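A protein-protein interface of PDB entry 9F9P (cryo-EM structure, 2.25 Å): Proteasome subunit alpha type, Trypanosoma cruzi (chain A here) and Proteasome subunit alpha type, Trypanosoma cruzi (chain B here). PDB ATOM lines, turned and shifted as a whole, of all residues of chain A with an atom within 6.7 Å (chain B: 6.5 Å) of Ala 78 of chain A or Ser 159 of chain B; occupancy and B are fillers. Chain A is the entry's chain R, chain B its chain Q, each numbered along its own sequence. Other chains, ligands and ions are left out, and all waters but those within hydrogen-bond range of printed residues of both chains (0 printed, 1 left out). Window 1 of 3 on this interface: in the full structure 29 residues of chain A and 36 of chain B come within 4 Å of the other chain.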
ATOM      1  N   LYS A  61     -24.997  15.327  -7.210  1.00  0.00           N
ATOM      2  CA  LYS A  61     -25.915  16.441  -7.455  1.00  0.00           C
ATOM      3  C   LYS A  61     -26.772  16.786  -6.233  1.00  0.00           C
ATOM      4  O   LYS A  61     -27.736  17.550  -6.341  1.00  0.00           O
ATOM      5  CB  LYS A  61     -26.847  16.089  -8.617  1.00  0.00           C
ATOM      6  CG  LYS A  61     -26.144  16.010  -9.964  1.00  0.00           C
ATOM      7  CD  LYS A  61     -25.355  17.281 -10.329  1.00  0.00           C
ATOM      8  CE  LYS A  61     -24.800  17.236 -11.735  1.00  0.00           C
ATOM      9  NZ  LYS A  61     -24.409  18.586 -12.190  1.00  0.00           N
ATOM     10  N   PHE A  73     -31.392  20.233  -6.180  1.00  0.00           N
ATOM     11  CA  PHE A  73     -31.934  21.289  -7.020  1.00  0.00           C
ATOM     12  C   PHE A  73     -32.464  20.806  -8.370  1.00  0.00           C
ATOM     13  O   PHE A  73     -32.224  19.692  -8.792  1.00  0.00           O
ATOM     14  CB  PHE A  73     -30.844  22.327  -7.276  1.00  0.00           C
ATOM     15  CG  PHE A  73     -29.828  21.817  -8.250  1.00  0.00           C
ATOM     16  CD1 PHE A  73     -28.792  21.016  -7.829  1.00  0.00           C
ATOM     17  CD2 PHE A  73     -29.974  22.058  -9.607  1.00  0.00           C
ATOM     18  CE1 PHE A  73     -27.902  20.482  -8.747  1.00  0.00           C
ATOM     19  CE2 PHE A  73     -29.101  21.500 -10.534  1.00  0.00           C
ATOM     20  CZ  PHE A  73     -28.070  20.705 -10.100  1.00  0.00           C
ATOM     21  N   GLY A  75     -32.863  22.790 -12.498  1.00  0.00           N
ATOM     22  CA  GLY A  75     -32.607  23.948 -13.344  1.00  0.00           C
ATOM     23  C   GLY A  75     -31.186  23.921 -13.900  1.00  0.00           C
ATOM     24  O   GLY A  75     -30.697  22.869 -14.276  1.00  0.00           O
ATOM     25  N   LEU A  76     -30.534  25.069 -13.979  1.00  0.00           N
ATOM     26  CA  LEU A  76     -29.198  25.142 -14.558  1.00  0.00           C
ATOM     27  C   LEU A  76     -28.162  24.735 -13.514  1.00  0.00           C
ATOM     28  O   LEU A  76     -27.970  25.459 -12.523  1.00  0.00           O
ATOM     29  CB  LEU A  76     -28.935  26.578 -15.037  1.00  0.00           C
ATOM     30  CG  LEU A  76     -29.998  27.144 -15.987  1.00  0.00           C
ATOM     31  CD1 LEU A  76     -29.548  28.457 -16.590  1.00  0.00           C
ATOM     32  CD2 LEU A  76     -30.314  26.144 -17.081  1.00  0.00           C
ATOM     33  N   SER A  77     -27.474  23.621 -13.786  1.00  0.00           N
ATOM     34  CA  SER A  77     -26.520  23.054 -12.858  1.00  0.00           C
ATOM     35  C   SER A  77     -25.387  24.012 -12.518  1.00  0.00           C
ATOM     36  O   SER A  77     -24.955  24.063 -11.374  1.00  0.00           O
ATOM     37  CB  SER A  77     -25.971  21.734 -13.344  1.00  0.00           C
ATOM     38  OG  SER A  77     -25.835  21.723 -14.749  1.00  0.00           O
ATOM     39  N   ALA A  78     -24.966  24.852 -13.455  1.00  0.00           N
ATOM     40  CA  ALA A  78     -23.837  25.729 -13.178  1.00  0.00           C
ATOM     41  C   ALA A  78     -24.240  26.885 -12.274  1.00  0.00           C
ATOM     42  O   ALA A  78     -23.430  27.310 -11.445  1.00  0.00           O
ATOM     43  CB  ALA A  78     -23.223  26.218 -14.467  1.00  0.00           C
ATOM     44  N   ASP A  79     -25.480  27.381 -12.409  1.00  0.00           N
ATOM     45  CA  ASP A  79     -26.000  28.413 -11.514  1.00  0.00           C
ATOM     46  C   ASP A  79     -26.167  27.861 -10.092  1.00  0.00           C
ATOM     47  O   ASP A  79     -25.970  28.588  -9.110  1.00  0.00           O
ATOM     48  CB  ASP A  79     -27.340  28.965 -12.006  1.00  0.00           C
ATOM     49  CG  ASP A  79     -27.374  29.832 -13.269  1.00  0.00           C
ATOM     50  OD1 ASP A  79     -26.335  29.898 -14.044  1.00  0.00           O
ATOM     51  OD2 ASP A  79     -28.468  30.441 -13.521  1.00  0.00           O
ATOM     52  N   ALA A  80     -26.516  26.570  -9.963  1.00  0.00           N
ATOM     53  CA  ALA A  80     -26.732  25.963  -8.660  1.00  0.00           C
ATOM     54  C   ALA A  80     -25.451  25.829  -7.853  1.00  0.00           C
ATOM     55  O   ALA A  80     -25.472  26.033  -6.645  1.00  0.00           O
ATOM     56  CB  ALA A  80     -27.340  24.618  -8.793  1.00  0.00           C
ATOM     57  N   ARG A  81     -24.360  25.495  -8.521  1.00  0.00           N
ATOM     58  CA  ARG A  81     -23.034  25.436  -7.924  1.00  0.00           C
ATOM     59  C   ARG A  81     -22.595  26.777  -7.329  1.00  0.00           C
ATOM     60  O   ARG A  81     -21.993  26.820  -6.270  1.00  0.00           O
ATOM     61  CB  ARG A  81     -22.058  25.008  -9.010  1.00  0.00           C
ATOM     62  CG  ARG A  81     -21.275  23.771  -8.678  1.00  0.00           C
ATOM     63  CD  ARG A  81     -20.301  23.318  -9.748  1.00  0.00           C
ATOM     64  NE  ARG A  81     -19.784  24.367 -10.600  1.00  0.00           N
ATOM     65  CZ  ARG A  81     -19.993  24.378 -11.905  1.00  0.00           C
ATOM     66  NH1 ARG A  81     -19.630  25.425 -12.618  1.00  0.00           N
ATOM     67  NH2 ARG A  81     -20.634  23.368 -12.468  1.00  0.00           N
ATOM     68  N   VAL A  82     -22.919  27.885  -7.971  1.00  0.00           N
ATOM     69  CA  VAL A  82     -22.628  29.196  -7.412  1.00  0.00           C
ATOM     70  C   VAL A  82     -23.428  29.457  -6.135  1.00  0.00           C
ATOM     71  O   VAL A  82     -22.881  30.039  -5.213  1.00  0.00           O
ATOM     72  CB  VAL A  82     -22.857  30.315  -8.457  1.00  0.00           C
ATOM     73  CG1 VAL A  82     -22.828  31.702  -7.846  1.00  0.00           C
ATOM     74  CG2 VAL A  82     -21.835  30.264  -9.547  1.00  0.00           C
ATOM     75  N   LEU A  83     -24.721  29.117  -6.113  1.00  0.00           N
ATOM     76  CA  LEU A  83     -25.583  29.275  -4.941  1.00  0.00           C
ATOM     77  C   LEU A  83     -25.110  28.408  -3.774  1.00  0.00           C
ATOM     78  O   LEU A  83     -25.168  28.831  -2.640  1.00  0.00           O
ATOM     79  CB  LEU A  83     -26.981  28.798  -5.333  1.00  0.00           C
ATOM     80  CG  LEU A  83     -28.168  29.722  -5.097  1.00  0.00           C
ATOM     81  CD1 LEU A  83     -27.801  31.152  -5.400  1.00  0.00           C
ATOM     82  CD2 LEU A  83     -29.344  29.302  -5.973  1.00  0.00           C
ATOM     83  N   VAL A 129     -32.890  28.356 -11.121  1.00  0.00           N
ATOM     84  CA  VAL A 129     -32.654  27.297 -10.161  1.00  0.00           C
ATOM     85  C   VAL A 129     -33.777  27.284  -9.137  1.00  0.00           C
ATOM     86  O   VAL A 129     -34.083  28.313  -8.563  1.00  0.00           O
ATOM     87  CB  VAL A 129     -31.360  27.590  -9.386  1.00  0.00           C
ATOM     88  CG1 VAL A 129     -31.210  26.713  -8.175  1.00  0.00           C
ATOM     89  CG2 VAL A 129     -30.125  27.460 -10.250  1.00  0.00           C
ATOM     90  N   VAL B  21     -24.805  31.017 -25.278  1.00  0.00           N
ATOM     91  CA  VAL B  21     -24.226  29.766 -24.788  1.00  0.00           C
ATOM     92  C   VAL B  21     -24.497  28.631 -25.771  1.00  0.00           C
ATOM     93  O   VAL B  21     -23.590  27.883 -26.065  1.00  0.00           O
ATOM     94  CB  VAL B  21     -24.743  29.448 -23.367  1.00  0.00           C
ATOM     95  CG1 VAL B  21     -24.327  28.080 -22.862  1.00  0.00           C
ATOM     96  CG2 VAL B  21     -24.299  30.494 -22.365  1.00  0.00           C
ATOM     97  N   GLU B  25     -21.588  26.602 -28.277  1.00  0.00           N
ATOM     98  CA  GLU B  25     -21.518  25.149 -28.352  1.00  0.00           C
ATOM     99  C   GLU B  25     -21.461  24.644 -29.795  1.00  0.00           C
ATOM    100  O   GLU B  25     -20.746  23.689 -30.073  1.00  0.00           O
ATOM    101  CB  GLU B  25     -22.676  24.509 -27.593  1.00  0.00           C
ATOM    102  CG  GLU B  25     -22.545  22.997 -27.430  1.00  0.00           C
ATOM    103  CD  GLU B  25     -23.768  22.311 -26.820  1.00  0.00           C
ATOM    104  OE1 GLU B  25     -23.899  21.062 -26.969  1.00  0.00           O
ATOM    105  OE2 GLU B  25     -24.600  23.017 -26.190  1.00  0.00           O
ATOM    106  N   CYS B 121     -14.696  25.977 -14.452  1.00  0.00           N
ATOM    107  CA  CYS B 121     -16.087  26.050 -14.851  1.00  0.00           C
ATOM    108  C   CYS B 121     -16.813  27.229 -14.212  1.00  0.00           C
ATOM    109  O   CYS B 121     -17.743  27.742 -14.791  1.00  0.00           O
ATOM    110  CB  CYS B 121     -16.744  24.721 -14.534  1.00  0.00           C
ATOM    111  SG  CYS B 121     -16.267  23.488 -15.778  1.00  0.00           S
ATOM    112  N   ASP B 122     -16.390  27.674 -13.032  1.00  0.00           N
ATOM    113  CA  ASP B 122     -16.980  28.836 -12.396  1.00  0.00           C
ATOM    114  C   ASP B 122     -16.571  30.114 -13.121  1.00  0.00           C
ATOM    115  O   ASP B 122     -17.339  31.073 -13.194  1.00  0.00           O
ATOM    116  CB  ASP B 122     -16.625  28.868 -10.903  1.00  0.00           C
ATOM    117  CG  ASP B 122     -17.420  27.862 -10.052  1.00  0.00           C
ATOM    118  OD1 ASP B 122     -18.375  27.222 -10.583  1.00  0.00           O
ATOM    119  OD2 ASP B 122     -17.089  27.710  -8.845  1.00  0.00           O
ATOM    120  N   LYS B 124     -16.161  30.169 -16.361  1.00  0.00           N
ATOM    121  CA  LYS B 124     -17.089  30.226 -17.477  1.00  0.00           C
ATOM    122  C   LYS B 124     -18.511  30.630 -17.085  1.00  0.00           C
ATOM    123  O   LYS B 124     -19.142  31.396 -17.789  1.00  0.00           O
ATOM    124  CB  LYS B 124     -17.177  28.880 -18.143  1.00  0.00           C
ATOM    125  CG  LYS B 124     -15.837  28.420 -18.701  1.00  0.00           C
ATOM    126  CD  LYS B 124     -16.050  27.294 -19.631  1.00  0.00           C
ATOM    127  CE  LYS B 124     -14.912  26.325 -19.685  1.00  0.00           C
ATOM    128  NZ  LYS B 124     -15.215  25.347 -20.753  1.00  0.00           N
ATOM    129  N   GLN B 125     -19.063  30.075 -16.019  1.00  0.00           N
ATOM    130  CA  GLN B 125     -20.401  30.447 -15.615  1.00  0.00           C
ATOM    131  C   GLN B 125     -20.546  31.971 -15.407  1.00  0.00           C
ATOM    132  O   GLN B 125     -21.599  32.516 -15.690  1.00  0.00           O
ATOM    133  CB  GLN B 125     -20.780  29.664 -14.353  1.00  0.00           C
ATOM    134  CG  GLN B 125     -22.257  29.776 -13.994  1.00  0.00           C
ATOM    135  CD  GLN B 125     -22.602  31.014 -13.213  1.00  0.00           C
ATOM    136  OE1 GLN B 125     -21.761  31.643 -12.591  1.00  0.00           O
ATOM    137  NE2 GLN B 125     -23.865  31.377 -13.220  1.00  0.00           N
ATOM    138  N   THR B 128     -21.702  34.091 -18.329  1.00  0.00           N
ATOM    139  CA  THR B 128     -23.083  33.881 -18.754  1.00  0.00           C
ATOM    140  C   THR B 128     -24.113  34.597 -17.894  1.00  0.00           C
ATOM    141  O   THR B 128     -25.285  34.570 -18.216  1.00  0.00           O
ATOM    142  CB  THR B 128     -23.476  32.396 -18.727  1.00  0.00           C
ATOM    143  OG1 THR B 128     -23.655  31.912 -17.395  1.00  0.00           O
ATOM    144  CG2 THR B 128     -22.431  31.541 -19.421  1.00  0.00           C
ATOM    145  N   ASP B 157     -17.895  22.036 -20.647  1.00  0.00           N
ATOM    146  CA  ASP B 157     -18.574  22.592 -21.821  1.00  0.00           C
ATOM    147  C   ASP B 157     -18.771  24.114 -21.696  1.00  0.00           C
ATOM    148  O   ASP B 157     -18.333  24.717 -20.718  1.00  0.00           O
ATOM    149  CB  ASP B 157     -19.899  21.885 -22.065  1.00  0.00           C
ATOM    150  CG  ASP B 157     -20.995  22.365 -21.135  1.00  0.00           C
ATOM    151  OD1 ASP B 157     -20.762  23.368 -20.430  1.00  0.00           O
ATOM    152  OD2 ASP B 157     -22.078  21.734 -21.123  1.00  0.00           O
ATOM    153  N   THR B 158     -19.426  24.731 -22.699  1.00  0.00           N
ATOM    154  CA  THR B 158     -19.498  26.189 -22.784  1.00  0.00           C
ATOM    155  C   THR B 158     -20.445  26.796 -21.752  1.00  0.00           C
ATOM    156  O   THR B 158     -20.254  27.958 -21.401  1.00  0.00           O
ATOM    157  CB  THR B 158     -19.853  26.668 -24.197  1.00  0.00           C
ATOM    158  OG1 THR B 158     -21.124  26.151 -24.593  1.00  0.00           O
ATOM    159  CG2 THR B 158     -18.835  26.220 -25.218  1.00  0.00           C
ATOM    160  N   SER B 159     -21.357  26.000 -21.171  1.00  0.00           N
ATOM    161  CA  SER B 159     -22.233  26.465 -20.095  1.00  0.00           C
ATOM    162  C   SER B 159     -21.566  26.492 -18.721  1.00  0.00           C
ATOM    163  O   SER B 159     -22.130  27.061 -17.793  1.00  0.00           O
ATOM    164  CB  SER B 159     -23.501  25.649 -20.020  1.00  0.00           C
ATOM    165  OG  SER B 159     -23.203  24.275 -20.109  1.00  0.00           O
ATOM    166  N   GLY B 160     -20.399  25.851 -18.566  1.00  0.00           N
ATOM    167  CA  GLY B 160     -19.766  25.754 -17.256  1.00  0.00           C
ATOM    168  C   GLY B 160     -20.137  24.484 -16.486  1.00  0.00           C
ATOM    169  O   GLY B 160     -19.995  24.450 -15.275  1.00  0.00           O
ATOM    170  N   ASN B 161     -20.632  23.475 -17.199  1.00  0.00           N
ATOM    171  CA  ASN B 161     -20.873  22.143 -16.680  1.00  0.00           C
ATOM    172  C   ASN B 161     -19.718  21.201 -16.978  1.00  0.00           C
ATOM    173  O   ASN B 161     -19.057  21.352 -17.993  1.00  0.00           O
ATOM    174  CB  ASN B 161     -22.129  21.555 -17.307  1.00  0.00           C
ATOM    175  CG  ASN B 161     -23.306  22.081 -16.540  1.00  0.00           C
ATOM    176  OD1 ASN B 161     -23.324  21.919 -15.323  1.00  0.00           O
ATOM    177  ND2 ASN B 161     -24.205  22.799 -17.199  1.00  0.00           N
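The guanidinium group of Arg 81 of chain A is in salt-bridge range of the side-chain carboxylate of Asp 122 of chain B (3.0 Å).
NE2 of Gln 125 of chain B is in hydrogen-bond range of OD1 of Asp 79 of chain A, at 3.0 Å.
The backbone carbonyl oxygen (O) of Gly 160 of chain B sits at hydrogen-bond distance from the guanidinium group (NH1) of Arg 81 of chain A (2.9 Å).
The side-chain amide oxygen (OD1) of Asn 161 of chain B lies within hydrogen-bond range of the side-chain hydroxyl (OG) of Ser 77 of chain A (2.6 Å).
The side-chain hydroxyl (OG1) of Thr 128 of chain B is in hydrogen-bond range of the backbone carbonyl oxygen (O) of Gln 125 of chain B (2.7 Å).
The side-chain carboxylate of Asp 157 of chain B sits at hydrogen-bond distance from the side-chain hydroxyl of Ser 159 of chain B.
The side-chain carboxylate of Asp 157 of chain B sits at hydrogen-bond distance from the backbone NH of Gly 160 of chain B (3.1 Å).
The backbone NH (N) of Asn 161 of chain B is in hydrogen-bond range of the side-chain carboxylate (OD1) of Asp 157 of chain B, at 3.2 Å.
The side-chain amide nitrogen (ND2) of Asn 161 of chain B lies within hydrogen-bond range of the side-chain hydroxyl (OG) of Ser 159 of chain B, 3.4 Å away.
Among the printed residues, pairs that only touch across the chains: Ala 78 of chain A with Gln 125 of chain B, Ala 78 of chain A with Ser 159 of chain B, Ala 78 of chain A with Gly 160 of chain B, Ala 78 of chain A with Asn 161 of chain B, Arg 81 of chain A with Cys 121 of chain B and Val 82 of chain A with Gln 125 of chain B.
Printed residues of chain B within 4 Å of Asp 79 of chain A: Gln 125 (3.0 Å).
Of the printed residues of chain A, Cys 121 of chain B touches Arg 81 (3.5 Å).
Of the printed residues of chain A, Gly 160 of chain B touches Ala 78 and Arg 81.
The nearest residue of chain A that does not touch Ser 159 of chain B is Arg 81 of chain A (6.0 Å).
Along chain B the printed residues that touch a printed residue of chain A span positions 121 to 161.
Among the printed residues, Asp or Glu carboxylates within 4 Å of a Lys or Arg side-chain nitrogen of the other chain: Arg 81 of chain A with Asp 122 of chain B (3.0 Å).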
